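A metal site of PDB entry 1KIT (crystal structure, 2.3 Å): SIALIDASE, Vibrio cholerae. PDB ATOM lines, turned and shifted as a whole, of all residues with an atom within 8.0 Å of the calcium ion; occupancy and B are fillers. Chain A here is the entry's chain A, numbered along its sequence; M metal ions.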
ATOM      1  N   VAL A 222     -29.139 -26.262 -29.017  1.00  0.00           N
ATOM      2  CA  VAL A 222     -29.669 -25.980 -30.342  1.00  0.00           C
ATOM      3  C   VAL A 222     -29.053 -26.954 -31.353  1.00  0.00           C
ATOM      4  O   VAL A 222     -27.888 -26.806 -31.802  1.00  0.00           O
ATOM      5  CB  VAL A 222     -29.426 -24.497 -30.740  1.00  0.00           C
ATOM      6  CG1 VAL A 222     -30.094 -24.187 -32.057  1.00  0.00           C
ATOM      7  CG2 VAL A 222     -29.970 -23.576 -29.657  1.00  0.00           C
ATOM      8  N   GLY A 224     -29.720 -30.219 -30.550  1.00  0.00           N
ATOM      9  CA  GLY A 224     -29.890 -31.372 -29.667  1.00  0.00           C
ATOM     10  C   GLY A 224     -28.547 -32.063 -29.574  1.00  0.00           C
ATOM     11  O   GLY A 224     -27.664 -31.767 -30.361  1.00  0.00           O
ATOM     12  N   GLY A 225     -28.371 -32.953 -28.602  1.00  0.00           N
ATOM     13  CA  GLY A 225     -27.099 -33.698 -28.487  1.00  0.00           C
ATOM     14  C   GLY A 225     -26.015 -33.116 -27.526  1.00  0.00           C
ATOM     15  O   GLY A 225     -25.960 -31.892 -27.261  1.00  0.00           O
ATOM     16  N   ASP A 226     -25.171 -34.008 -27.036  1.00  0.00           N
ATOM     17  CA  ASP A 226     -24.061 -33.664 -26.149  1.00  0.00           C
ATOM     18  C   ASP A 226     -23.089 -32.717 -26.798  1.00  0.00           C
ATOM     19  O   ASP A 226     -22.920 -32.691 -28.000  1.00  0.00           O
ATOM     20  CB  ASP A 226     -23.270 -34.926 -25.777  1.00  0.00           C
ATOM     21  CG  ASP A 226     -24.101 -35.920 -25.025  1.00  0.00           C
ATOM     22  OD1 ASP A 226     -25.017 -35.470 -24.281  1.00  0.00           O
ATOM     23  OD2 ASP A 226     -23.843 -37.128 -25.181  1.00  0.00           O
ATOM     24  N   PRO A 227     -22.444 -31.922 -25.955  1.00  0.00           N
ATOM     25  CA  PRO A 227     -21.461 -30.978 -26.409  1.00  0.00           C
ATOM     26  C   PRO A 227     -20.405 -31.701 -27.252  1.00  0.00           C
ATOM     27  O   PRO A 227     -20.167 -32.885 -27.058  1.00  0.00           O
ATOM     28  CB  PRO A 227     -20.850 -30.438 -25.109  1.00  0.00           C
ATOM     29  CG  PRO A 227     -21.271 -31.313 -24.062  1.00  0.00           C
ATOM     30  CD  PRO A 227     -22.522 -32.014 -24.492  1.00  0.00           C
ATOM     31  N   GLY A 228     -19.843 -30.993 -28.222  1.00  0.00           N
ATOM     32  CA  GLY A 228     -18.828 -31.552 -29.095  1.00  0.00           C
ATOM     33  C   GLY A 228     -19.374 -31.848 -30.465  1.00  0.00           C
ATOM     34  O   GLY A 228     -18.618 -32.049 -31.388  1.00  0.00           O
ATOM     35  N   ALA A 229     -20.701 -31.792 -30.646  1.00  0.00           N
ATOM     36  CA  ALA A 229     -21.249 -32.024 -31.996  1.00  0.00           C
ATOM     37  C   ALA A 229     -21.082 -30.861 -32.908  1.00  0.00           C
ATOM     38  O   ALA A 229     -21.414 -29.733 -32.588  1.00  0.00           O
ATOM     39  CB  ALA A 229     -22.717 -32.492 -31.986  1.00  0.00           C
ATOM     40  N   LEU A 230     -20.561 -31.135 -34.080  1.00  0.00           N
ATOM     41  CA  LEU A 230     -20.428 -30.111 -35.068  1.00  0.00           C
ATOM     42  C   LEU A 230     -21.835 -29.599 -35.363  1.00  0.00           C
ATOM     43  O   LEU A 230     -22.019 -28.532 -35.937  1.00  0.00           O
ATOM     44  CB  LEU A 230     -19.885 -30.727 -36.326  1.00  0.00           C
ATOM     45  CG  LEU A 230     -19.410 -29.700 -37.324  1.00  0.00           C
ATOM     46  CD1 LEU A 230     -17.929 -29.357 -37.079  1.00  0.00           C
ATOM     47  CD2 LEU A 230     -19.643 -30.212 -38.704  1.00  0.00           C
ATOM     48  N   SER A 231     -22.820 -30.424 -35.020  1.00  0.00           N
ATOM     49  CA  SER A 231     -24.211 -30.118 -35.303  1.00  0.00           C
ATOM     50  C   SER A 231     -24.966 -29.629 -34.086  1.00  0.00           C
ATOM     51  O   SER A 231     -26.045 -30.101 -33.797  1.00  0.00           O
ATOM     52  CB  SER A 231     -24.910 -31.326 -35.901  1.00  0.00           C
ATOM     53  OG  SER A 231     -25.036 -32.354 -34.929  1.00  0.00           O
ATOM     54  N   ASN A 232     -24.407 -28.658 -33.375  1.00  0.00           N
ATOM     55  CA  ASN A 232     -25.098 -28.051 -32.247  1.00  0.00           C
ATOM     56  C   ASN A 232     -24.336 -26.894 -31.697  1.00  0.00           C
ATOM     57  O   ASN A 232     -23.189 -26.673 -32.045  1.00  0.00           O
ATOM     58  CB  ASN A 232     -25.493 -29.076 -31.148  1.00  0.00           C
ATOM     59  CG  ASN A 232     -24.273 -29.608 -30.325  1.00  0.00           C
ATOM     60  OD1 ASN A 232     -23.254 -28.937 -30.187  1.00  0.00           O
ATOM     61  ND2 ASN A 232     -24.420 -30.801 -29.754  1.00  0.00           N
ATOM     62  N   THR A 233     -24.978 -26.160 -30.822  1.00  0.00           N
ATOM     63  CA  THR A 233     -24.350 -25.060 -30.129  1.00  0.00           C
ATOM     64  C   THR A 233     -25.086 -25.120 -28.852  1.00  0.00           C
ATOM     65  O   THR A 233     -26.331 -25.036 -28.827  1.00  0.00           O
ATOM     66  CB  THR A 233     -24.630 -23.718 -30.788  1.00  0.00           C
ATOM     67  OG1 THR A 233     -24.095 -23.724 -32.124  1.00  0.00           O
ATOM     68  CG2 THR A 233     -23.987 -22.604 -29.961  1.00  0.00           C
ATOM     69  N   ASN A 234     -24.370 -25.449 -27.783  1.00  0.00           N
ATOM     70  CA  ASN A 234     -25.024 -25.587 -26.526  1.00  0.00           C
ATOM     71  C   ASN A 234     -24.704 -24.422 -25.650  1.00  0.00           C
ATOM     72  O   ASN A 234     -23.566 -23.928 -25.677  1.00  0.00           O
ATOM     73  CB  ASN A 234     -24.696 -26.928 -25.891  1.00  0.00           C
ATOM     74  CG  ASN A 234     -25.133 -28.095 -26.780  1.00  0.00           C
ATOM     75  OD1 ASN A 234     -25.812 -27.890 -27.766  1.00  0.00           O
ATOM     76  ND2 ASN A 234     -24.735 -29.339 -26.420  1.00  0.00           N
ATOM     77  N   ASN A 259     -20.491 -16.568 -26.095  1.00  0.00           N
ATOM     78  CA  ASN A 259     -20.230 -17.298 -27.325  1.00  0.00           C
ATOM     79  C   ASN A 259     -20.777 -16.545 -28.531  1.00  0.00           C
ATOM     80  O   ASN A 259     -21.812 -16.914 -29.117  1.00  0.00           O
ATOM     81  CB  ASN A 259     -20.817 -18.699 -27.175  1.00  0.00           C
ATOM     82  CG  ASN A 259     -20.423 -19.656 -28.297  1.00  0.00           C
ATOM     83  OD1 ASN A 259     -19.466 -19.409 -29.069  1.00  0.00           O
ATOM     84  ND2 ASN A 259     -21.111 -20.767 -28.394  1.00  0.00           N
ATOM     85  N   ASP A 262     -20.782 -18.576 -31.685  1.00  0.00           N
ATOM     86  CA  ASP A 262     -21.278 -19.910 -31.388  1.00  0.00           C
ATOM     87  C   ASP A 262     -20.207 -20.900 -31.708  1.00  0.00           C
ATOM     88  O   ASP A 262     -20.454 -22.016 -32.155  1.00  0.00           O
ATOM     89  CB  ASP A 262     -22.521 -20.184 -32.237  1.00  0.00           C
ATOM     90  CG  ASP A 262     -23.554 -19.063 -32.118  1.00  0.00           C
ATOM     91  OD1 ASP A 262     -23.469 -18.242 -31.182  1.00  0.00           O
ATOM     92  OD2 ASP A 262     -24.382 -18.952 -33.061  1.00  0.00           O
ATOM     93  N   GLU A 263     -19.000 -20.469 -31.362  1.00  0.00           N
ATOM     94  CA  GLU A 263     -17.812 -21.223 -31.550  1.00  0.00           C
ATOM     95  C   GLU A 263     -17.662 -22.216 -30.404  1.00  0.00           C
ATOM     96  O   GLU A 263     -16.870 -23.170 -30.513  1.00  0.00           O
ATOM     97  CB  GLU A 263     -16.635 -20.258 -31.558  1.00  0.00           C
ATOM     98  CG  GLU A 263     -15.350 -20.866 -31.924  1.00  0.00           C
ATOM     99  CD  GLU A 263     -14.243 -19.875 -31.827  1.00  0.00           C
ATOM    100  OE1 GLU A 263     -14.538 -18.672 -31.576  1.00  0.00           O
ATOM    101  OE2 GLU A 263     -13.069 -20.251 -32.000  1.00  0.00           O
ATOM    102  N   PHE A 264     -18.417 -22.063 -29.344  1.00  0.00           N
ATOM    103  CA  PHE A 264     -18.282 -22.958 -28.238  1.00  0.00           C
ATOM    104  C   PHE A 264     -19.540 -23.733 -27.920  1.00  0.00           C
ATOM    105  O   PHE A 264     -20.584 -23.573 -28.543  1.00  0.00           O
ATOM    106  CB  PHE A 264     -17.778 -22.209 -26.996  1.00  0.00           C
ATOM    107  CG  PHE A 264     -16.530 -21.390 -27.246  1.00  0.00           C
ATOM    108  CD1 PHE A 264     -15.292 -22.010 -27.448  1.00  0.00           C
ATOM    109  CD2 PHE A 264     -16.598 -20.001 -27.256  1.00  0.00           C
ATOM    110  CE1 PHE A 264     -14.122 -21.253 -27.643  1.00  0.00           C
ATOM    111  CE2 PHE A 264     -15.440 -19.221 -27.496  1.00  0.00           C
ATOM    112  CZ  PHE A 264     -14.215 -19.847 -27.702  1.00  0.00           C
ATOM    113  N   ASP A 265     -19.420 -24.624 -26.973  1.00  0.00           N
ATOM    114  CA  ASP A 265     -20.548 -25.371 -26.474  1.00  0.00           C
ATOM    115  C   ASP A 265     -20.348 -25.219 -24.985  1.00  0.00           C
ATOM    116  O   ASP A 265     -19.202 -25.230 -24.513  1.00  0.00           O
ATOM    117  CB  ASP A 265     -20.432 -26.860 -26.845  1.00  0.00           C
ATOM    118  CG  ASP A 265     -21.165 -27.213 -28.134  1.00  0.00           C
ATOM    119  OD1 ASP A 265     -21.926 -26.383 -28.669  1.00  0.00           O
ATOM    120  OD2 ASP A 265     -20.986 -28.342 -28.627  1.00  0.00           O
ATOM    121  N   PHE A 266     -21.415 -24.979 -24.231  1.00  0.00           N
ATOM    122  CA  PHE A 266     -21.245 -24.920 -22.795  1.00  0.00           C
ATOM    123  C   PHE A 266     -21.984 -26.084 -22.191  1.00  0.00           C
ATOM    124  O   PHE A 266     -22.900 -26.642 -22.802  1.00  0.00           O
ATOM    125  CB  PHE A 266     -21.662 -23.581 -22.212  1.00  0.00           C
ATOM    126  CG  PHE A 266     -20.877 -22.431 -22.765  1.00  0.00           C
ATOM    127  CD1 PHE A 266     -21.155 -21.922 -24.013  1.00  0.00           C
ATOM    128  CD2 PHE A 266     -19.784 -21.935 -22.064  1.00  0.00           C
ATOM    129  CE1 PHE A 266     -20.403 -20.855 -24.526  1.00  0.00           C
ATOM    130  CE2 PHE A 266     -19.004 -20.937 -22.565  1.00  0.00           C
ATOM    131  CZ  PHE A 266     -19.330 -20.346 -23.778  1.00  0.00           C
ATOM    132  N   TRP A 287     -16.268 -25.912 -24.243  1.00  0.00           N
ATOM    133  CA  TRP A 287     -15.568 -26.818 -25.156  1.00  0.00           C
ATOM    134  C   TRP A 287     -15.702 -26.107 -26.505  1.00  0.00           C
ATOM    135  O   TRP A 287     -16.539 -25.218 -26.640  1.00  0.00           O
ATOM    136  CB  TRP A 287     -16.335 -28.165 -25.226  1.00  0.00           C
ATOM    137  CG  TRP A 287     -16.796 -28.700 -23.886  1.00  0.00           C
ATOM    138  CD1 TRP A 287     -17.936 -28.384 -23.238  1.00  0.00           C
ATOM    139  CD2 TRP A 287     -16.115 -29.643 -23.050  1.00  0.00           C
ATOM    140  NE1 TRP A 287     -18.005 -29.048 -22.052  1.00  0.00           N
ATOM    141  CE2 TRP A 287     -16.885 -29.813 -21.889  1.00  0.00           C
ATOM    142  CE3 TRP A 287     -14.914 -30.356 -23.158  1.00  0.00           C
ATOM    143  CZ2 TRP A 287     -16.495 -30.643 -20.837  1.00  0.00           C
ATOM    144  CZ3 TRP A 287     -14.542 -31.208 -22.121  1.00  0.00           C
ATOM    145  CH2 TRP A 287     -15.326 -31.340 -20.970  1.00  0.00           C
ATOM    146  N   PRO A 288     -14.927 -26.500 -27.492  1.00  0.00           N
ATOM    147  CA  PRO A 288     -15.146 -25.906 -28.814  1.00  0.00           C
ATOM    148  C   PRO A 288     -16.415 -26.611 -29.283  1.00  0.00           C
ATOM    149  O   PRO A 288     -16.732 -27.711 -28.794  1.00  0.00           O
ATOM    150  CB  PRO A 288     -13.967 -26.410 -29.647  1.00  0.00           C
ATOM    151  CG  PRO A 288     -13.521 -27.658 -28.932  1.00  0.00           C
ATOM    152  CD  PRO A 288     -13.720 -27.328 -27.461  1.00  0.00           C
ATOM    153  N   THR A 289     -17.146 -26.003 -30.200  1.00  0.00           N
ATOM    154  CA  THR A 289     -18.378 -26.608 -30.647  1.00  0.00           C
ATOM    155  C   THR A 289     -18.167 -27.989 -31.285  1.00  0.00           C
ATOM    156  O   THR A 289     -19.086 -28.777 -31.347  1.00  0.00           O
ATOM    157  CB  THR A 289     -19.125 -25.687 -31.597  1.00  0.00           C
ATOM    158  OG1 THR A 289     -20.470 -26.169 -31.770  1.00  0.00           O
ATOM    159  CG2 THR A 289     -18.415 -25.631 -32.963  1.00  0.00           C
ATOM    160  N   ASP A 290     -16.960 -28.308 -31.714  1.00  0.00           N
ATOM    161  CA  ASP A 290     -16.750 -29.589 -32.366  1.00  0.00           C
ATOM    162  C   ASP A 290     -16.045 -30.696 -31.599  1.00  0.00           C
ATOM    163  O   ASP A 290     -15.832 -31.775 -32.143  1.00  0.00           O
ATOM    164  CB  ASP A 290     -16.098 -29.408 -33.753  1.00  0.00           C
ATOM    165  CG  ASP A 290     -14.768 -28.699 -33.675  1.00  0.00           C
ATOM    166  OD1 ASP A 290     -14.453 -28.235 -32.551  1.00  0.00           O
ATOM    167  OD2 ASP A 290     -14.048 -28.620 -34.703  1.00  0.00           O
ATOM    168  N   ALA A 291     -15.605 -30.436 -30.377  1.00  0.00           N
ATOM    169  CA  ALA A 291     -14.933 -31.495 -29.625  1.00  0.00           C
ATOM    170  C   ALA A 291     -15.074 -31.284 -28.141  1.00  0.00           C
ATOM    171  O   ALA A 291     -15.084 -30.146 -27.654  1.00  0.00           O
ATOM    172  CB  ALA A 291     -13.475 -31.613 -30.008  1.00  0.00           C
HETATM  173 CA    CA M   1     -21.405 -28.021 -30.898  1.00  0.00          CA
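The side-chain amide nitrogen (ND2) of Asn 232 lies within hydrogen-bond range of the backbone carbonyl oxygen (O) of Asp 226, at 3.0 Å.
The side-chain carboxylate of Asp 265 lies close to the backbone NH of Asn 234 (2.8 Å).
N of Gly 228 sits close to OD2 of Asp 265 (2.9 Å).
The side-chain amide nitrogen (ND2) of Asn 232 lies within hydrogen-bond range of the backbone carbonyl oxygen (O) of Gly 225 (3.1 Å).
The backbone carbonyl oxygen (O) of Trp 287 is in hydrogen-bond range of the backbone NH (N) of Asp 265, at 3.0 Å.
The side-chain amide nitrogen of Asn 232 lies within hydrogen-bond range of the backbone carbonyl oxygen of Gly 224 (3.4 Å).
N of Thr 289 lies within hydrogen-bond range of O of Glu 263.
The calcium ion is bound by the side-chain amide oxygen (OD1) of Asn 232 (2.2 Å), the side-chain hydroxyl (OG1) of Thr 289 (2.3 Å), the side-chain carboxylate (OD2) of Asp 265 (2.3 Å), the backbone carbonyl oxygen (O) of Ala 229 (2.4 Å), the backbone carbonyl oxygen (O) of Thr 289 (2.5 Å), the backbone carbonyl oxygen (O) of Asn 232 (2.5 Å) and the side-chain carboxylate (OD1) of Asp 265 (2.8 Å).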
